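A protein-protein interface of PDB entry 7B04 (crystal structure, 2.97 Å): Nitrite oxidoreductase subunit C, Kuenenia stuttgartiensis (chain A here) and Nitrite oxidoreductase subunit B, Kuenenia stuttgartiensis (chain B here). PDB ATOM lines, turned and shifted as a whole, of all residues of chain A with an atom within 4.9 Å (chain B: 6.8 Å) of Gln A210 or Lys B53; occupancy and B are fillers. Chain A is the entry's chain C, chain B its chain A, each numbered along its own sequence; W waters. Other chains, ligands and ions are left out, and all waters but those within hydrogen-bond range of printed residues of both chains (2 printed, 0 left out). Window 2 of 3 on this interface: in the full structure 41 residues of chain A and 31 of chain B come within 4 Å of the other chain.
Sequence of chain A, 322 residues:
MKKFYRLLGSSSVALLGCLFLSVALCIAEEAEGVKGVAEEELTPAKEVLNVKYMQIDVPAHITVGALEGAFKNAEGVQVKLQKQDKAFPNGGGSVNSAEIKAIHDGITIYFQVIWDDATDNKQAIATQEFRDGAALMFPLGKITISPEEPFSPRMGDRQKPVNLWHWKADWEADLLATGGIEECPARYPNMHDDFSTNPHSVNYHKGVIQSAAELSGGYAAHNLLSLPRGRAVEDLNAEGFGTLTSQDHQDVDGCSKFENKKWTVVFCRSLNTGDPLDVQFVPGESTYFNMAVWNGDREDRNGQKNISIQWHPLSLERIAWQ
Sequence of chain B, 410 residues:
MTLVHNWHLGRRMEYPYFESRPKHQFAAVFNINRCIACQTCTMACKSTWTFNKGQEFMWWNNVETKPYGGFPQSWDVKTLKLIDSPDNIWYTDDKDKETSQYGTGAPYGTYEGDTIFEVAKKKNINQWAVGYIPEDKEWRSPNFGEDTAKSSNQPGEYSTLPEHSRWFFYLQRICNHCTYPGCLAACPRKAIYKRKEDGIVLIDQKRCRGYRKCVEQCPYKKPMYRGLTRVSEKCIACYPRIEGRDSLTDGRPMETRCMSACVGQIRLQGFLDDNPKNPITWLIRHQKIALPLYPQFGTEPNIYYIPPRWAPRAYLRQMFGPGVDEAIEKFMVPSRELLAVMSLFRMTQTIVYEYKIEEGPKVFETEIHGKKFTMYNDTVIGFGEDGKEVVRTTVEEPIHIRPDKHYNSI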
ATOM      1  N   GLU A 183     -13.999 -12.472   7.479  1.00  0.00           N
ATOM      2  CA  GLU A 183     -15.197 -12.023   6.788  1.00  0.00           C
ATOM      3  C   GLU A 183     -15.918 -10.970   7.629  1.00  0.00           C
ATOM      4  O   GLU A 183     -15.530 -10.673   8.762  1.00  0.00           O
ATOM      5  CB  GLU A 183     -16.088 -13.216   6.433  1.00  0.00           C
ATOM      6  CG  GLU A 183     -15.316 -14.317   5.709  1.00  0.00           C
ATOM      7  CD  GLU A 183     -16.198 -15.221   4.869  1.00  0.00           C
ATOM      8  OE1 GLU A 183     -17.426 -14.997   4.837  1.00  0.00           O
ATOM      9  OE2 GLU A 183     -15.659 -16.154   4.235  1.00  0.00           O
ATOM     10  N   CYS A 184     -16.979 -10.406   7.051  1.00  0.00           N
ATOM     11  CA  CYS A 184     -17.601  -9.208   7.617  1.00  0.00           C
ATOM     12  C   CYS A 184     -18.026  -9.312   9.082  1.00  0.00           C
ATOM     13  O   CYS A 184     -17.821  -8.327   9.812  1.00  0.00           O
ATOM     14  CB  CYS A 184     -18.798  -8.806   6.745  1.00  0.00           C
ATOM     15  SG  CYS A 184     -18.330  -8.319   5.073  1.00  0.00           S
ATOM     16  N   SER A 196     -27.143 -14.957   4.293  1.00  0.00           N
ATOM     17  CA  SER A 196     -25.861 -15.389   4.814  1.00  0.00           C
ATOM     18  C   SER A 196     -25.911 -15.652   6.312  1.00  0.00           C
ATOM     19  O   SER A 196     -25.085 -16.424   6.808  1.00  0.00           O
ATOM     20  CB  SER A 196     -24.769 -14.365   4.488  1.00  0.00           C
ATOM     21  OG  SER A 196     -24.927 -13.164   5.225  1.00  0.00           O
ATOM     22  N   HIS A 205     -29.916 -23.792  -1.731  1.00  0.00           N
ATOM     23  CA  HIS A 205     -30.024 -22.341  -1.824  1.00  0.00           C
ATOM     24  C   HIS A 205     -28.688 -21.688  -1.510  1.00  0.00           C
ATOM     25  O   HIS A 205     -28.154 -20.918  -2.313  1.00  0.00           O
ATOM     26  CB  HIS A 205     -31.108 -21.815  -0.876  1.00  0.00           C
ATOM     27  CG  HIS A 205     -31.227 -20.313  -0.889  1.00  0.00           C
ATOM     28  ND1 HIS A 205     -30.769 -19.518   0.148  1.00  0.00           N
ATOM     29  CD2 HIS A 205     -31.725 -19.470  -1.828  1.00  0.00           C
ATOM     30  CE1 HIS A 205     -30.998 -18.255  -0.147  1.00  0.00           C
ATOM     31  NE2 HIS A 205     -31.575 -18.202  -1.335  1.00  0.00           N
ATOM     32  N   LYS A 206     -28.126 -22.006  -0.348  1.00  0.00           N
ATOM     33  CA  LYS A 206     -26.821 -21.472   0.032  1.00  0.00           C
ATOM     34  C   LYS A 206     -25.730 -21.893  -0.953  1.00  0.00           C
ATOM     35  O   LYS A 206     -24.791 -21.127  -1.210  1.00  0.00           O
ATOM     36  CB  LYS A 206     -26.459 -21.926   1.453  1.00  0.00           C
ATOM     37  CG  LYS A 206     -25.364 -21.112   2.124  1.00  0.00           C
ATOM     38  CD  LYS A 206     -25.284 -21.501   3.603  1.00  0.00           C
ATOM     39  CE  LYS A 206     -24.641 -20.401   4.437  1.00  0.00           C
ATOM     40  NZ  LYS A 206     -25.519 -20.020   5.583  1.00  0.00           N
ATOM     41  N   GLY A 207     -25.821 -23.112  -1.490  1.00  0.00           N
ATOM     42  CA  GLY A 207     -24.829 -23.562  -2.449  1.00  0.00           C
ATOM     43  C   GLY A 207     -24.782 -22.705  -3.699  1.00  0.00           C
ATOM     44  O   GLY A 207     -23.704 -22.412  -4.219  1.00  0.00           O
ATOM     45  N   VAL A 208     -25.947 -22.299  -4.199  1.00  0.00           N
ATOM     46  CA  VAL A 208     -25.999 -21.438  -5.376  1.00  0.00           C
ATOM     47  C   VAL A 208     -25.618 -20.006  -5.021  1.00  0.00           C
ATOM     48  O   VAL A 208     -24.821 -19.367  -5.718  1.00  0.00           O
ATOM     49  CB  VAL A 208     -27.391 -21.511  -6.031  1.00  0.00           C
ATOM     50  CG1 VAL A 208     -27.531 -20.445  -7.107  1.00  0.00           C
ATOM     51  CG2 VAL A 208     -27.621 -22.893  -6.617  1.00  0.00           C
ATOM     52  N   ILE A 209     -26.180 -19.478  -3.931  1.00  0.00           N
ATOM     53  CA  ILE A 209     -25.996 -18.065  -3.609  1.00  0.00           C
ATOM     54  C   ILE A 209     -24.543 -17.772  -3.261  1.00  0.00           C
ATOM     55  O   ILE A 209     -23.977 -16.763  -3.699  1.00  0.00           O
ATOM     56  CB  ILE A 209     -26.944 -17.649  -2.469  1.00  0.00           C
ATOM     57  CG1 ILE A 209     -28.401 -17.755  -2.921  1.00  0.00           C
ATOM     58  CG2 ILE A 209     -26.631 -16.236  -2.002  1.00  0.00           C
ATOM     59  CD1 ILE A 209     -28.739 -16.875  -4.103  1.00  0.00           C
ATOM     60  N   GLN A 210     -23.909 -18.645  -2.479  1.00  0.00           N
ATOM     61  CA  GLN A 210     -22.516 -18.467  -2.098  1.00  0.00           C
ATOM     62  C   GLN A 210     -21.564 -19.276  -2.971  1.00  0.00           C
ATOM     63  O   GLN A 210     -20.442 -19.572  -2.547  1.00  0.00           O
ATOM     64  CB  GLN A 210     -22.322 -18.807  -0.620  1.00  0.00           C
ATOM     65  CG  GLN A 210     -23.060 -17.857   0.313  1.00  0.00           C
ATOM     66  CD  GLN A 210     -22.675 -18.034   1.767  1.00  0.00           C
ATOM     67  OE1 GLN A 210     -21.791 -18.825   2.096  1.00  0.00           O
ATOM     68  NE2 GLN A 210     -23.339 -17.294   2.648  1.00  0.00           N
ATOM     69  N   SER A 211     -21.990 -19.641  -4.176  1.00  0.00           N
ATOM     70  CA  SER A 211     -21.075 -20.191  -5.162  1.00  0.00           C
ATOM     71  C   SER A 211     -20.127 -19.103  -5.658  1.00  0.00           C
ATOM     72  O   SER A 211     -20.409 -17.905  -5.563  1.00  0.00           O
ATOM     73  CB  SER A 211     -21.844 -20.805  -6.332  1.00  0.00           C
ATOM     74  OG  SER A 211     -22.578 -19.819  -7.036  1.00  0.00           O
ATOM     75  N   ALA A 212     -18.983 -19.538  -6.193  1.00  0.00           N
ATOM     76  CA  ALA A 212     -17.966 -18.589  -6.639  1.00  0.00           C
ATOM     77  C   ALA A 212     -18.508 -17.645  -7.708  1.00  0.00           C
ATOM     78  O   ALA A 212     -18.234 -16.440  -7.675  1.00  0.00           O
ATOM     79  CB  ALA A 212     -16.740 -19.342  -7.158  1.00  0.00           C
ATOM     80  N   LEU A 215     -20.748 -15.205  -5.931  1.00  0.00           N
ATOM     81  CA  LEU A 215     -20.093 -14.306  -4.966  1.00  0.00           C
ATOM     82  C   LEU A 215     -19.636 -13.061  -5.727  1.00  0.00           C
ATOM     83  O   LEU A 215     -19.872 -11.972  -5.235  1.00  0.00           O
ATOM     84  CB  LEU A 215     -18.949 -15.074  -4.313  1.00  0.00           C
ATOM     85  CG  LEU A 215     -19.339 -15.893  -3.090  1.00  0.00           C
ATOM     86  CD1 LEU A 215     -18.252 -16.854  -2.699  1.00  0.00           C
ATOM     87  CD2 LEU A 215     -19.669 -14.995  -1.926  1.00  0.00           C
ATOM     88  N   THR B  50     -25.682  -6.818  -5.959  1.00  0.00           N
ATOM     89  CA  THR B  50     -25.140  -6.474  -4.649  1.00  0.00           C
ATOM     90  C   THR B  50     -25.890  -7.185  -3.528  1.00  0.00           C
ATOM     91  O   THR B  50     -26.125  -6.618  -2.459  1.00  0.00           O
ATOM     92  CB  THR B  50     -25.172  -4.963  -4.430  1.00  0.00           C
ATOM     93  OG1 THR B  50     -26.458  -4.580  -3.927  1.00  0.00           O
ATOM     94  CG2 THR B  50     -24.910  -4.224  -5.734  1.00  0.00           C
ATOM     95  N   PHE B  51     -26.248  -8.448  -3.745  1.00  0.00           N
ATOM     96  CA  PHE B  51     -27.119  -9.176  -2.831  1.00  0.00           C
ATOM     97  C   PHE B  51     -26.361 -10.095  -1.881  1.00  0.00           C
ATOM     98  O   PHE B  51     -26.992 -10.739  -1.036  1.00  0.00           O
ATOM     99  CB  PHE B  51     -28.157  -9.987  -3.619  1.00  0.00           C
ATOM    100  CG  PHE B  51     -27.580 -11.141  -4.390  1.00  0.00           C
ATOM    101  CD1 PHE B  51     -27.048 -10.953  -5.655  1.00  0.00           C
ATOM    102  CD2 PHE B  51     -27.586 -12.420  -3.854  1.00  0.00           C
ATOM    103  CE1 PHE B  51     -26.522 -12.014  -6.366  1.00  0.00           C
ATOM    104  CE2 PHE B  51     -27.060 -13.484  -4.559  1.00  0.00           C
ATOM    105  CZ  PHE B  51     -26.529 -13.282  -5.818  1.00  0.00           C
ATOM    106  N   ASN B  52     -25.040 -10.171  -1.990  1.00  0.00           N
ATOM    107  CA  ASN B  52     -24.256 -11.190  -1.313  1.00  0.00           C
ATOM    108  C   ASN B  52     -23.390 -10.567  -0.216  1.00  0.00           C
ATOM    109  O   ASN B  52     -23.508  -9.378   0.104  1.00  0.00           O
ATOM    110  CB  ASN B  52     -23.416 -11.961  -2.333  1.00  0.00           C
ATOM    111  CG  ASN B  52     -23.255 -13.423  -1.968  1.00  0.00           C
ATOM    112  OD1 ASN B  52     -23.541 -13.831  -0.842  1.00  0.00           O
ATOM    113  ND2 ASN B  52     -22.802 -14.222  -2.926  1.00  0.00           N
ATOM    114  N   LYS B  53     -22.520 -11.391   0.366  1.00  0.00           N
ATOM    115  CA  LYS B  53     -21.714 -10.976   1.508  1.00  0.00           C
ATOM    116  C   LYS B  53     -20.764  -9.842   1.140  1.00  0.00           C
ATOM    117  O   LYS B  53     -20.220  -9.794   0.034  1.00  0.00           O
ATOM    118  CB  LYS B  53     -20.916 -12.165   2.047  1.00  0.00           C
ATOM    119  CG  LYS B  53     -21.768 -13.300   2.590  1.00  0.00           C
ATOM    120  CD  LYS B  53     -20.911 -14.344   3.286  1.00  0.00           C
ATOM    121  CE  LYS B  53     -20.052 -15.105   2.289  1.00  0.00           C
ATOM    122  NZ  LYS B  53     -19.264 -16.187   2.943  1.00  0.00           N
ATOM    123  N   GLY B  54     -20.565  -8.926   2.088  1.00  0.00           N
ATOM    124  CA  GLY B  54     -19.706  -7.776   1.898  1.00  0.00           C
ATOM    125  C   GLY B  54     -20.340  -6.582   1.222  1.00  0.00           C
ATOM    126  O   GLY B  54     -19.748  -5.495   1.248  1.00  0.00           O
ATOM    127  N   GLN B  55     -21.519  -6.736   0.621  1.00  0.00           N
ATOM    128  CA  GLN B  55     -22.198  -5.655  -0.087  1.00  0.00           C
ATOM    129  C   GLN B  55     -23.515  -5.286   0.585  1.00  0.00           C
ATOM    130  O   GLN B  55     -24.428  -4.775  -0.067  1.00  0.00           O
ATOM    131  CB  GLN B  55     -22.434  -6.035  -1.546  1.00  0.00           C
ATOM    132  CG  GLN B  55     -21.424  -7.023  -2.060  1.00  0.00           C
ATOM    133  CD  GLN B  55     -21.844  -7.689  -3.349  1.00  0.00           C
ATOM    134  OE1 GLN B  55     -22.640  -8.626  -3.347  1.00  0.00           O
ATOM    135  NE2 GLN B  55     -21.298  -7.215  -4.463  1.00  0.00           N
ATOM    136  N   GLU B  56     -23.615  -5.524   1.892  1.00  0.00           N
ATOM    137  CA  GLU B  56     -24.877  -5.318   2.594  1.00  0.00           C
ATOM    138  C   GLU B  56     -25.268  -3.847   2.616  1.00  0.00           C
ATOM    139  O   GLU B  56     -26.462  -3.523   2.615  1.00  0.00           O
ATOM    140  CB  GLU B  56     -24.781  -5.879   4.012  1.00  0.00           C
ATOM    141  CG  GLU B  56     -24.507  -7.379   4.066  1.00  0.00           C
ATOM    142  CD  GLU B  56     -23.024  -7.709   4.033  1.00  0.00           C
ATOM    143  OE1 GLU B  56     -22.204  -6.769   3.951  1.00  0.00           O
ATOM    144  OE2 GLU B  56     -22.678  -8.909   4.086  1.00  0.00           O
ATOM    145  N   ARG B 226     -15.943  -3.224  -1.055  1.00  0.00           N
ATOM    146  CA  ARG B 226     -16.519  -4.476  -0.586  1.00  0.00           C
ATOM    147  C   ARG B 226     -15.615  -5.093   0.468  1.00  0.00           C
ATOM    148  O   ARG B 226     -14.502  -5.534   0.157  1.00  0.00           O
ATOM    149  CB  ARG B 226     -16.733  -5.451  -1.739  1.00  0.00           C
ATOM    150  CG  ARG B 226     -17.647  -6.602  -1.375  1.00  0.00           C
ATOM    151  CD  ARG B 226     -18.024  -7.448  -2.572  1.00  0.00           C
ATOM    152  NE  ARG B 226     -18.670  -8.678  -2.136  1.00  0.00           N
ATOM    153  CZ  ARG B 226     -18.877  -9.735  -2.912  1.00  0.00           C
ATOM    154  NH1 ARG B 226     -18.478  -9.736  -4.180  1.00  0.00           N
ATOM    155  NH2 ARG B 226     -19.482 -10.804  -2.415  1.00  0.00           N
ATOM    156  N   GLY B 227     -16.056  -5.027   1.722  1.00  0.00           N
ATOM    157  CA  GLY B 227     -15.282  -5.606   2.812  1.00  0.00           C
ATOM    158  C   GLY B 227     -14.812  -7.029   2.568  1.00  0.00           C
ATOM    159  O   GLY B 227     -13.674  -7.376   2.891  1.00  0.00           O
ATOM    160  N   LEU B 228     -15.667  -7.865   1.977  1.00  0.00           N
ATOM    161  CA  LEU B 228     -15.318  -9.275   1.785  1.00  0.00           C
ATOM    162  C   LEU B 228     -14.175  -9.469   0.789  1.00  0.00           C
ATOM    163  O   LEU B 228     -13.236 -10.231   1.046  1.00  0.00           O
ATOM    164  CB  LEU B 228     -16.551 -10.065   1.330  1.00  0.00           C
ATOM    165  CG  LEU B 228     -16.439 -11.587   1.494  1.00  0.00           C
ATOM    166  CD1 LEU B 228     -16.820 -12.001   2.910  1.00  0.00           C
ATOM    167  CD2 LEU B 228     -17.302 -12.294   0.457  1.00  0.00           C
ATOM    168  N   THR B 229     -14.242  -8.802  -0.360  1.00  0.00           N
ATOM    169  CA  THR B 229     -13.273  -9.012  -1.431  1.00  0.00           C
ATOM    170  C   THR B 229     -12.064  -8.092  -1.333  1.00  0.00           C
ATOM    171  O   THR B 229     -11.127  -8.242  -2.126  1.00  0.00           O
ATOM    172  CB  THR B 229     -13.951  -8.828  -2.794  1.00  0.00           C
ATOM    173  OG1 THR B 229     -14.601  -7.551  -2.842  1.00  0.00           O
ATOM    174  CG2 THR B 229     -14.980  -9.925  -3.023  1.00  0.00           C
HETATM  175  O   HOH W   1     -20.917 -10.873   5.111  1.00  0.00           O
HETATM  176  O   HOH W   2     -18.137  -4.934   4.203  1.00  0.00           O
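Of chain B, only Lys B53 (3.7 Å) comes within 4 Å of Gln A210. Of the printed residues of chain A, Lys B53 touches Glu A183 (2.9 Å), Ser A196 (3.7 Å) and Gln A210 (3.7 Å). Printed residues of chain B within 4 Å of Ser A196: Lys B53 (3.7 Å). Of the printed residues of chain B, Leu A215 touches Asn B52 and Arg B226. Of the printed residues of chain B, Ile A209 touches Phe B51 (3.8 Å) and Asn B52 (2.9 Å). Printed residues of chain A within 4 Å of Phe B51: Ile A209. Thr B50 touches none of the printed residues of chain A. Thr B229 touches none of the printed residues of chain A.
The backbone NH (N) of Gly B54 lies within hydrogen-bond range of the side-chain carboxylate (OE2) of Glu B56 (2.9 Å). N of Asn B52 is in hydrogen-bond range of OE1 of Gln B55. O of Lys B53 sits at hydrogen-bond distance from NH2 of Arg B226, at 2.7 Å.
Among the printed residues, 9 pairs touch across the chains. Among the printed residues, Asp or Glu carboxylates within 4 Å of a Lys or Arg side-chain nitrogen of the other chain: Glu A183 with Lys B53 (2.9 Å).
N of Gly B54 sits close to SG of Cys A184 (3.8 Å). The guanidinium group (NH1) of Arg B226 is in hydrogen-bond range of the backbone carbonyl oxygen (O) of Leu A215. OE1 of Glu A183 is in salt-bridge range of NZ of Lys B53, at 2.9 Å. The backbone carbonyl oxygen (O) of Ile A209 is in hydrogen-bond range of the side-chain amide nitrogen (ND2) of Asn B52.
Among the printed residues, pairs that only touch across the chains: Glu A183 with Leu B228, Ser A196 with Lys B53, Ile A209 with Phe B51, Gln A210 with Lys B53 and Leu A215 with Asn B52.
Water W1 lies within hydrogen-bond range of OE2 of Glu B56 (2.8 Å) and SG of Cys A184 (3.6 Å). Water W2 lies within hydrogen-bond range of the backbone NH of Gly B227 (3.2 Å), the backbone carbonyl oxygen of Gly B54 (3.4 Å) and the side-chain sulfur of Cys A184 (3.5 Å).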
